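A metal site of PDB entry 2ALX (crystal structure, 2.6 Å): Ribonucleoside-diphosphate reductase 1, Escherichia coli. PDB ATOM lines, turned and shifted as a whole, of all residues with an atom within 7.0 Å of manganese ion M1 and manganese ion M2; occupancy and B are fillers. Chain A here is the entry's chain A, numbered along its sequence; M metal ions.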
ATOM      1  N   GLN A  81       4.638 -34.305  27.253  1.00  0.00           N
ATOM      2  CA  GLN A  81       4.964 -33.574  26.034  1.00  0.00           C
ATOM      3  C   GLN A  81       3.972 -33.976  24.957  1.00  0.00           C
ATOM      4  O   GLN A  81       3.445 -33.129  24.230  1.00  0.00           O
ATOM      5  CB  GLN A  81       6.405 -33.878  25.594  1.00  0.00           C
ATOM      6  CG  GLN A  81       7.447 -33.609  26.686  1.00  0.00           C
ATOM      7  CD  GLN A  81       8.894 -33.659  26.194  1.00  0.00           C
ATOM      8  OE1 GLN A  81       9.299 -34.601  25.509  1.00  0.00           O
ATOM      9  NE2 GLN A  81       9.668 -32.647  26.554  1.00  0.00           N
ATOM     10  N   LEU A  84       0.585 -32.227  25.627  1.00  0.00           N
ATOM     11  CA  LEU A  84       0.635 -30.829  25.240  1.00  0.00           C
ATOM     12  C   LEU A  84       0.495 -30.661  23.752  1.00  0.00           C
ATOM     13  O   LEU A  84      -0.364 -29.908  23.302  1.00  0.00           O
ATOM     14  CB  LEU A  84       1.932 -30.198  25.723  1.00  0.00           C
ATOM     15  CG  LEU A  84       2.037 -29.962  27.233  1.00  0.00           C
ATOM     16  CD1 LEU A  84       3.301 -29.145  27.524  1.00  0.00           C
ATOM     17  CD2 LEU A  84       0.808 -29.213  27.719  1.00  0.00           C
ATOM     18  N   ASP A  85       1.310 -31.362  22.967  1.00  0.00           N
ATOM     19  CA  ASP A  85       1.252 -31.228  21.528  1.00  0.00           C
ATOM     20  C   ASP A  85       0.014 -31.873  20.910  1.00  0.00           C
ATOM     21  O   ASP A  85      -0.359 -31.528  19.794  1.00  0.00           O
ATOM     22  CB  ASP A  85       2.525 -31.754  20.856  1.00  0.00           C
ATOM     23  CG  ASP A  85       3.678 -30.735  20.892  1.00  0.00           C
ATOM     24  OD1 ASP A  85       3.406 -29.519  20.884  1.00  0.00           O
ATOM     25  OD2 ASP A  85       4.857 -31.146  20.904  1.00  0.00           O
ATOM     26  N   GLN A  88      -2.129 -28.829  21.361  1.00  0.00           N
ATOM     27  CA  GLN A  88      -1.658 -27.786  20.467  1.00  0.00           C
ATOM     28  C   GLN A  88      -1.779 -28.058  18.989  1.00  0.00           C
ATOM     29  O   GLN A  88      -1.856 -27.124  18.205  1.00  0.00           O
ATOM     30  CB  GLN A  88      -0.213 -27.421  20.790  1.00  0.00           C
ATOM     31  CG  GLN A  88      -0.010 -26.626  22.090  1.00  0.00           C
ATOM     32  CD  GLN A  88      -0.829 -25.350  22.140  1.00  0.00           C
ATOM     33  OE1 GLN A  88      -2.009 -25.375  22.448  1.00  0.00           O
ATOM     34  NE2 GLN A  88      -0.200 -24.223  21.819  1.00  0.00           N
ATOM     35  N   TRP A 112       1.725 -22.868  12.612  1.00  0.00           N
ATOM     36  CA  TRP A 112       2.021 -23.160  14.006  1.00  0.00           C
ATOM     37  C   TRP A 112       1.370 -24.495  14.436  1.00  0.00           C
ATOM     38  O   TRP A 112       2.034 -25.364  15.003  1.00  0.00           O
ATOM     39  CB  TRP A 112       1.540 -21.965  14.850  1.00  0.00           C
ATOM     40  CG  TRP A 112       1.449 -22.179  16.358  1.00  0.00           C
ATOM     41  CD1 TRP A 112       2.074 -23.153  17.093  1.00  0.00           C
ATOM     42  CD2 TRP A 112       0.722 -21.368  17.288  1.00  0.00           C
ATOM     43  NE1 TRP A 112       1.787 -22.995  18.425  1.00  0.00           N
ATOM     44  CE2 TRP A 112       0.951 -21.911  18.579  1.00  0.00           C
ATOM     45  CE3 TRP A 112      -0.109 -20.245  17.158  1.00  0.00           C
ATOM     46  CZ2 TRP A 112       0.385 -21.356  19.742  1.00  0.00           C
ATOM     47  CZ3 TRP A 112      -0.674 -19.690  18.322  1.00  0.00           C
ATOM     48  CH2 TRP A 112      -0.416 -20.248  19.595  1.00  0.00           C
ATOM     49  N   SER A 115       3.096 -27.426  12.618  1.00  0.00           N
ATOM     50  CA  SER A 115       4.348 -27.850  13.248  1.00  0.00           C
ATOM     51  C   SER A 115       4.121 -28.684  14.515  1.00  0.00           C
ATOM     52  O   SER A 115       4.907 -29.581  14.814  1.00  0.00           O
ATOM     53  CB  SER A 115       5.269 -26.649  13.539  1.00  0.00           C
ATOM     54  OG  SER A 115       4.679 -25.704  14.415  1.00  0.00           O
ATOM     55  N   GLU A 116       3.040 -28.439  15.236  1.00  0.00           N
ATOM     56  CA  GLU A 116       2.800 -29.236  16.439  1.00  0.00           C
ATOM     57  C   GLU A 116       2.448 -30.677  16.109  1.00  0.00           C
ATOM     58  O   GLU A 116       2.707 -31.578  16.919  1.00  0.00           O
ATOM     59  CB  GLU A 116       1.700 -28.604  17.302  1.00  0.00           C
ATOM     60  CG  GLU A 116       1.984 -27.156  17.667  1.00  0.00           C
ATOM     61  CD  GLU A 116       3.102 -26.975  18.693  1.00  0.00           C
ATOM     62  OE1 GLU A 116       3.987 -27.846  18.823  1.00  0.00           O
ATOM     63  OE2 GLU A 116       3.105 -25.914  19.360  1.00  0.00           O
ATOM     64  N   THR A 117       1.862 -30.925  14.931  1.00  0.00           N
ATOM     65  CA  THR A 117       1.508 -32.295  14.559  1.00  0.00           C
ATOM     66  C   THR A 117       2.785 -33.065  14.240  1.00  0.00           C
ATOM     67  O   THR A 117       2.885 -34.281  14.467  1.00  0.00           O
ATOM     68  CB  THR A 117       0.527 -32.348  13.343  1.00  0.00           C
ATOM     69  OG1 THR A 117       1.179 -31.885  12.155  1.00  0.00           O
ATOM     70  CG2 THR A 117      -0.677 -31.489  13.617  1.00  0.00           C
ATOM     71  N   HIS A 119       5.549 -32.598  15.785  1.00  0.00           N
ATOM     72  CA  HIS A 119       6.088 -32.940  17.096  1.00  0.00           C
ATOM     73  C   HIS A 119       5.349 -34.170  17.612  1.00  0.00           C
ATOM     74  O   HIS A 119       5.963 -35.103  18.136  1.00  0.00           O
ATOM     75  CB  HIS A 119       5.911 -31.773  18.081  1.00  0.00           C
ATOM     76  CG  HIS A 119       6.611 -30.523  17.679  1.00  0.00           C
ATOM     77  ND1 HIS A 119       6.509 -29.347  18.401  1.00  0.00           N
ATOM     78  CD2 HIS A 119       7.433 -30.249  16.634  1.00  0.00           C
ATOM     79  CE1 HIS A 119       7.232 -28.409  17.809  1.00  0.00           C
ATOM     80  NE2 HIS A 119       7.804 -28.935  16.737  1.00  0.00           N
ATOM     81  N   SER A 120       4.028 -34.205  17.478  1.00  0.00           N
ATOM     82  CA  SER A 120       3.267 -35.363  17.932  1.00  0.00           C
ATOM     83  C   SER A 120       3.848 -36.612  17.272  1.00  0.00           C
ATOM     84  O   SER A 120       4.090 -37.613  17.928  1.00  0.00           O
ATOM     85  CB  SER A 120       1.806 -35.227  17.531  1.00  0.00           C
ATOM     86  OG  SER A 120       1.240 -34.049  18.066  1.00  0.00           O
ATOM     87  N   TYR A 123       7.013 -37.770  18.735  1.00  0.00           N
ATOM     88  CA  TYR A 123       6.787 -38.492  19.976  1.00  0.00           C
ATOM     89  C   TYR A 123       6.384 -39.933  19.695  1.00  0.00           C
ATOM     90  O   TYR A 123       6.797 -40.841  20.399  1.00  0.00           O
ATOM     91  CB  TYR A 123       5.689 -37.829  20.820  1.00  0.00           C
ATOM     92  CG  TYR A 123       5.993 -36.416  21.241  1.00  0.00           C
ATOM     93  CD1 TYR A 123       7.297 -36.039  21.609  1.00  0.00           C
ATOM     94  CD2 TYR A 123       4.998 -35.444  21.248  1.00  0.00           C
ATOM     95  CE1 TYR A 123       7.586 -34.736  21.982  1.00  0.00           C
ATOM     96  CE2 TYR A 123       5.277 -34.140  21.610  1.00  0.00           C
ATOM     97  CZ  TYR A 123       6.569 -33.783  21.960  1.00  0.00           C
ATOM     98  OH  TYR A 123       6.855 -32.489  22.296  1.00  0.00           O
ATOM     99  N   LEU A 204       1.875 -22.164  28.333  1.00  0.00           N
ATOM    100  CA  LEU A 204       2.057 -23.535  27.895  1.00  0.00           C
ATOM    101  C   LEU A 204       3.281 -23.660  26.988  1.00  0.00           C
ATOM    102  O   LEU A 204       4.031 -24.635  27.074  1.00  0.00           O
ATOM    103  CB  LEU A 204       0.792 -23.999  27.166  1.00  0.00           C
ATOM    104  CG  LEU A 204       0.708 -25.466  26.712  1.00  0.00           C
ATOM    105  CD1 LEU A 204      -0.735 -25.802  26.340  1.00  0.00           C
ATOM    106  CD2 LEU A 204       1.636 -25.670  25.535  1.00  0.00           C
ATOM    107  N   GLU A 205       3.482 -22.672  26.131  1.00  0.00           N
ATOM    108  CA  GLU A 205       4.609 -22.684  25.213  1.00  0.00           C
ATOM    109  C   GLU A 205       5.875 -22.201  25.873  1.00  0.00           C
ATOM    110  O   GLU A 205       6.935 -22.790  25.688  1.00  0.00           O
ATOM    111  CB  GLU A 205       4.318 -21.791  23.988  1.00  0.00           C
ATOM    112  CG  GLU A 205       3.087 -22.177  23.154  1.00  0.00           C
ATOM    113  CD  GLU A 205       3.357 -23.191  22.060  1.00  0.00           C
ATOM    114  OE1 GLU A 205       4.519 -23.566  21.839  1.00  0.00           O
ATOM    115  OE2 GLU A 205       2.389 -23.631  21.404  1.00  0.00           O
ATOM    116  N   PHE A 209       6.382 -26.297  28.392  1.00  0.00           N
ATOM    117  CA  PHE A 209       7.310 -27.008  27.531  1.00  0.00           C
ATOM    118  C   PHE A 209       8.775 -26.942  27.937  1.00  0.00           C
ATOM    119  O   PHE A 209       9.488 -27.934  27.796  1.00  0.00           O
ATOM    120  CB  PHE A 209       7.173 -26.530  26.094  1.00  0.00           C
ATOM    121  CG  PHE A 209       6.303 -27.414  25.277  1.00  0.00           C
ATOM    122  CD1 PHE A 209       6.679 -28.717  25.010  1.00  0.00           C
ATOM    123  CD2 PHE A 209       5.058 -26.980  24.853  1.00  0.00           C
ATOM    124  CE1 PHE A 209       5.841 -29.578  24.339  1.00  0.00           C
ATOM    125  CE2 PHE A 209       4.203 -27.843  24.178  1.00  0.00           C
ATOM    126  CZ  PHE A 209       4.601 -29.151  23.919  1.00  0.00           C
ATOM    127  N   PHE A 213      11.918 -29.748  28.733  1.00  0.00           N
ATOM    128  CA  PHE A 213      13.192 -29.872  28.031  1.00  0.00           C
ATOM    129  C   PHE A 213      14.335 -30.013  29.019  1.00  0.00           C
ATOM    130  O   PHE A 213      15.375 -30.605  28.707  1.00  0.00           O
ATOM    131  CB  PHE A 213      13.463 -28.641  27.158  1.00  0.00           C
ATOM    132  CG  PHE A 213      12.402 -28.363  26.149  1.00  0.00           C
ATOM    133  CD1 PHE A 213      11.669 -29.402  25.584  1.00  0.00           C
ATOM    134  CD2 PHE A 213      12.145 -27.056  25.733  1.00  0.00           C
ATOM    135  CE1 PHE A 213      10.683 -29.150  24.619  1.00  0.00           C
ATOM    136  CE2 PHE A 213      11.175 -26.790  24.774  1.00  0.00           C
ATOM    137  CZ  PHE A 213      10.443 -27.842  24.208  1.00  0.00           C
ATOM    138  N   ILE A 235      12.319 -29.590  18.357  1.00  0.00           N
ATOM    139  CA  ILE A 235      11.014 -29.145  18.880  1.00  0.00           C
ATOM    140  C   ILE A 235      11.181 -27.819  19.638  1.00  0.00           C
ATOM    141  O   ILE A 235      10.364 -26.910  19.505  1.00  0.00           O
ATOM    142  CB  ILE A 235      10.373 -30.210  19.824  1.00  0.00           C
ATOM    143  CG1 ILE A 235      10.016 -31.476  19.043  1.00  0.00           C
ATOM    144  CG2 ILE A 235       9.121 -29.666  20.449  1.00  0.00           C
ATOM    145  CD1 ILE A 235       9.538 -32.615  19.901  1.00  0.00           C
ATOM    146  N   ASP A 238      11.346 -24.815  17.553  1.00  0.00           N
ATOM    147  CA  ASP A 238       9.997 -24.443  17.117  1.00  0.00           C
ATOM    148  C   ASP A 238       9.186 -23.748  18.207  1.00  0.00           C
ATOM    149  O   ASP A 238       8.567 -22.717  17.963  1.00  0.00           O
ATOM    150  CB  ASP A 238       9.194 -25.653  16.668  1.00  0.00           C
ATOM    151  CG  ASP A 238       9.677 -26.234  15.376  1.00  0.00           C
ATOM    152  OD1 ASP A 238      10.146 -25.465  14.519  1.00  0.00           O
ATOM    153  OD2 ASP A 238       9.570 -27.464  15.224  1.00  0.00           O
ATOM    154  N   GLU A 239       9.186 -24.347  19.399  1.00  0.00           N
ATOM    155  CA  GLU A 239       8.403 -23.779  20.496  1.00  0.00           C
ATOM    156  C   GLU A 239       8.890 -22.376  20.765  1.00  0.00           C
ATOM    157  O   GLU A 239       8.178 -21.553  21.323  1.00  0.00           O
ATOM    158  CB  GLU A 239       8.514 -24.657  21.754  1.00  0.00           C
ATOM    159  CG  GLU A 239       8.240 -26.168  21.562  1.00  0.00           C
ATOM    160  CD  GLU A 239       6.814 -26.516  21.144  1.00  0.00           C
ATOM    161  OE1 GLU A 239       5.952 -25.605  21.053  1.00  0.00           O
ATOM    162  OE2 GLU A 239       6.526 -27.712  20.911  1.00  0.00           O
ATOM    163  N   ALA A 240      10.119 -22.074  20.338  1.00  0.00           N
ATOM    164  CA  ALA A 240      10.666 -20.729  20.520  1.00  0.00           C
ATOM    165  C   ALA A 240       9.943 -19.801  19.545  1.00  0.00           C
ATOM    166  O   ALA A 240       9.593 -18.667  19.896  1.00  0.00           O
ATOM    167  CB  ALA A 240      12.152 -20.717  20.256  1.00  0.00           C
ATOM    168  N   HIS A 242       6.966 -20.289  18.411  1.00  0.00           N
ATOM    169  CA  HIS A 242       5.622 -20.233  18.942  1.00  0.00           C
ATOM    170  C   HIS A 242       5.476 -19.238  20.074  1.00  0.00           C
ATOM    171  O   HIS A 242       4.542 -18.428  20.055  1.00  0.00           O
ATOM    172  CB  HIS A 242       5.174 -21.622  19.411  1.00  0.00           C
ATOM    173  CG  HIS A 242       5.228 -22.668  18.343  1.00  0.00           C
ATOM    174  ND1 HIS A 242       5.052 -24.011  18.609  1.00  0.00           N
ATOM    175  CD2 HIS A 242       5.446 -22.575  17.012  1.00  0.00           C
ATOM    176  CE1 HIS A 242       5.163 -24.694  17.486  1.00  0.00           C
ATOM    177  NE2 HIS A 242       5.411 -23.853  16.501  1.00  0.00           N
ATOM    178  N   LEU A 243       6.368 -19.265  21.050  1.00  0.00           N
ATOM    179  CA  LEU A 243       6.280 -18.323  22.155  1.00  0.00           C
ATOM    180  C   LEU A 243       6.532 -16.891  21.667  1.00  0.00           C
ATOM    181  O   LEU A 243       6.017 -15.939  22.251  1.00  0.00           O
ATOM    182  CB  LEU A 243       7.245 -18.692  23.288  1.00  0.00           C
ATOM    183  CG  LEU A 243       8.749 -18.444  23.144  1.00  0.00           C
ATOM    184  CD1 LEU A 243       9.067 -16.965  23.343  1.00  0.00           C
ATOM    185  CD2 LEU A 243       9.485 -19.281  24.189  1.00  0.00           C
HETATM  186 MN    MN M   1       5.123 -28.684  20.046  1.00  0.00          MN
HETATM  187 MN    MN M   2       4.260 -24.984  20.426  1.00  0.00          MN
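NE1 of Trp 112 lies close to OE2 of Glu 205, at 3.1 Å.
The backbone NH of Phe 209 lies within hydrogen-bond range of the backbone carbonyl oxygen of Leu 204 (3.2 Å).
A ring nitrogen (NE2) of His 242 lies within hydrogen-bond range of the side-chain hydroxyl of Ser 115 (2.9 Å).
The side-chain carboxylate of Glu 116 lies close to the indole nitrogen of Trp 112, at 3.3 Å.
OD2 of Asp 238 is in hydrogen-bond range of NE2 of His 119 (2.8 Å).
The backbone carbonyl oxygen of Asp 85 lies within hydrogen-bond range of the side-chain hydroxyl of Ser 120 (3.4 Å).
A ring nitrogen (ND1) of His 242 lies close to the indole nitrogen of Trp 112 (3.4 Å).
OH of Tyr 123 lies close to OD2 of Asp 85 (2.8 Å).
Residues that only touch manganese ion M1: Phe 209.
Five residues have an atom within 4 Å of manganese ion M1: Asp 85, Glu 116, His 119, Phe 209 and Glu 239.
Residues that only touch manganese ion M2: Trp 112 (3.8 Å).
Within 4 Å of manganese ion M2: Trp 112, Glu 116, Glu 205, Glu 239 and His 242.
The nearest printed residue that does not touch manganese ion M2 is Asp 85 (4.6 Å).
Manganese ion M1 is bound by OE1 of Glu 116 (1.9 Å).
Manganese ion M1 is bound by OE2 of Glu 239 (1.9 Å).
OD1 of Asp 85 binds manganese ion M1 (2.1 Å).
ND1 of His 119 binds manganese ion M1.
Manganese ion M1 is bound by OD2 of Asp 85, 2.6 Å away.
Manganese ion M1 has five donor atoms within binding distance.
Manganese ion M2 is bound by OE2 of Glu 116, OE1 of Glu 239, OE1 of Glu 205, ND1 of His 242 and OE2 of Glu 205.
Manganese ion M2 has five donor atoms within binding distance.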
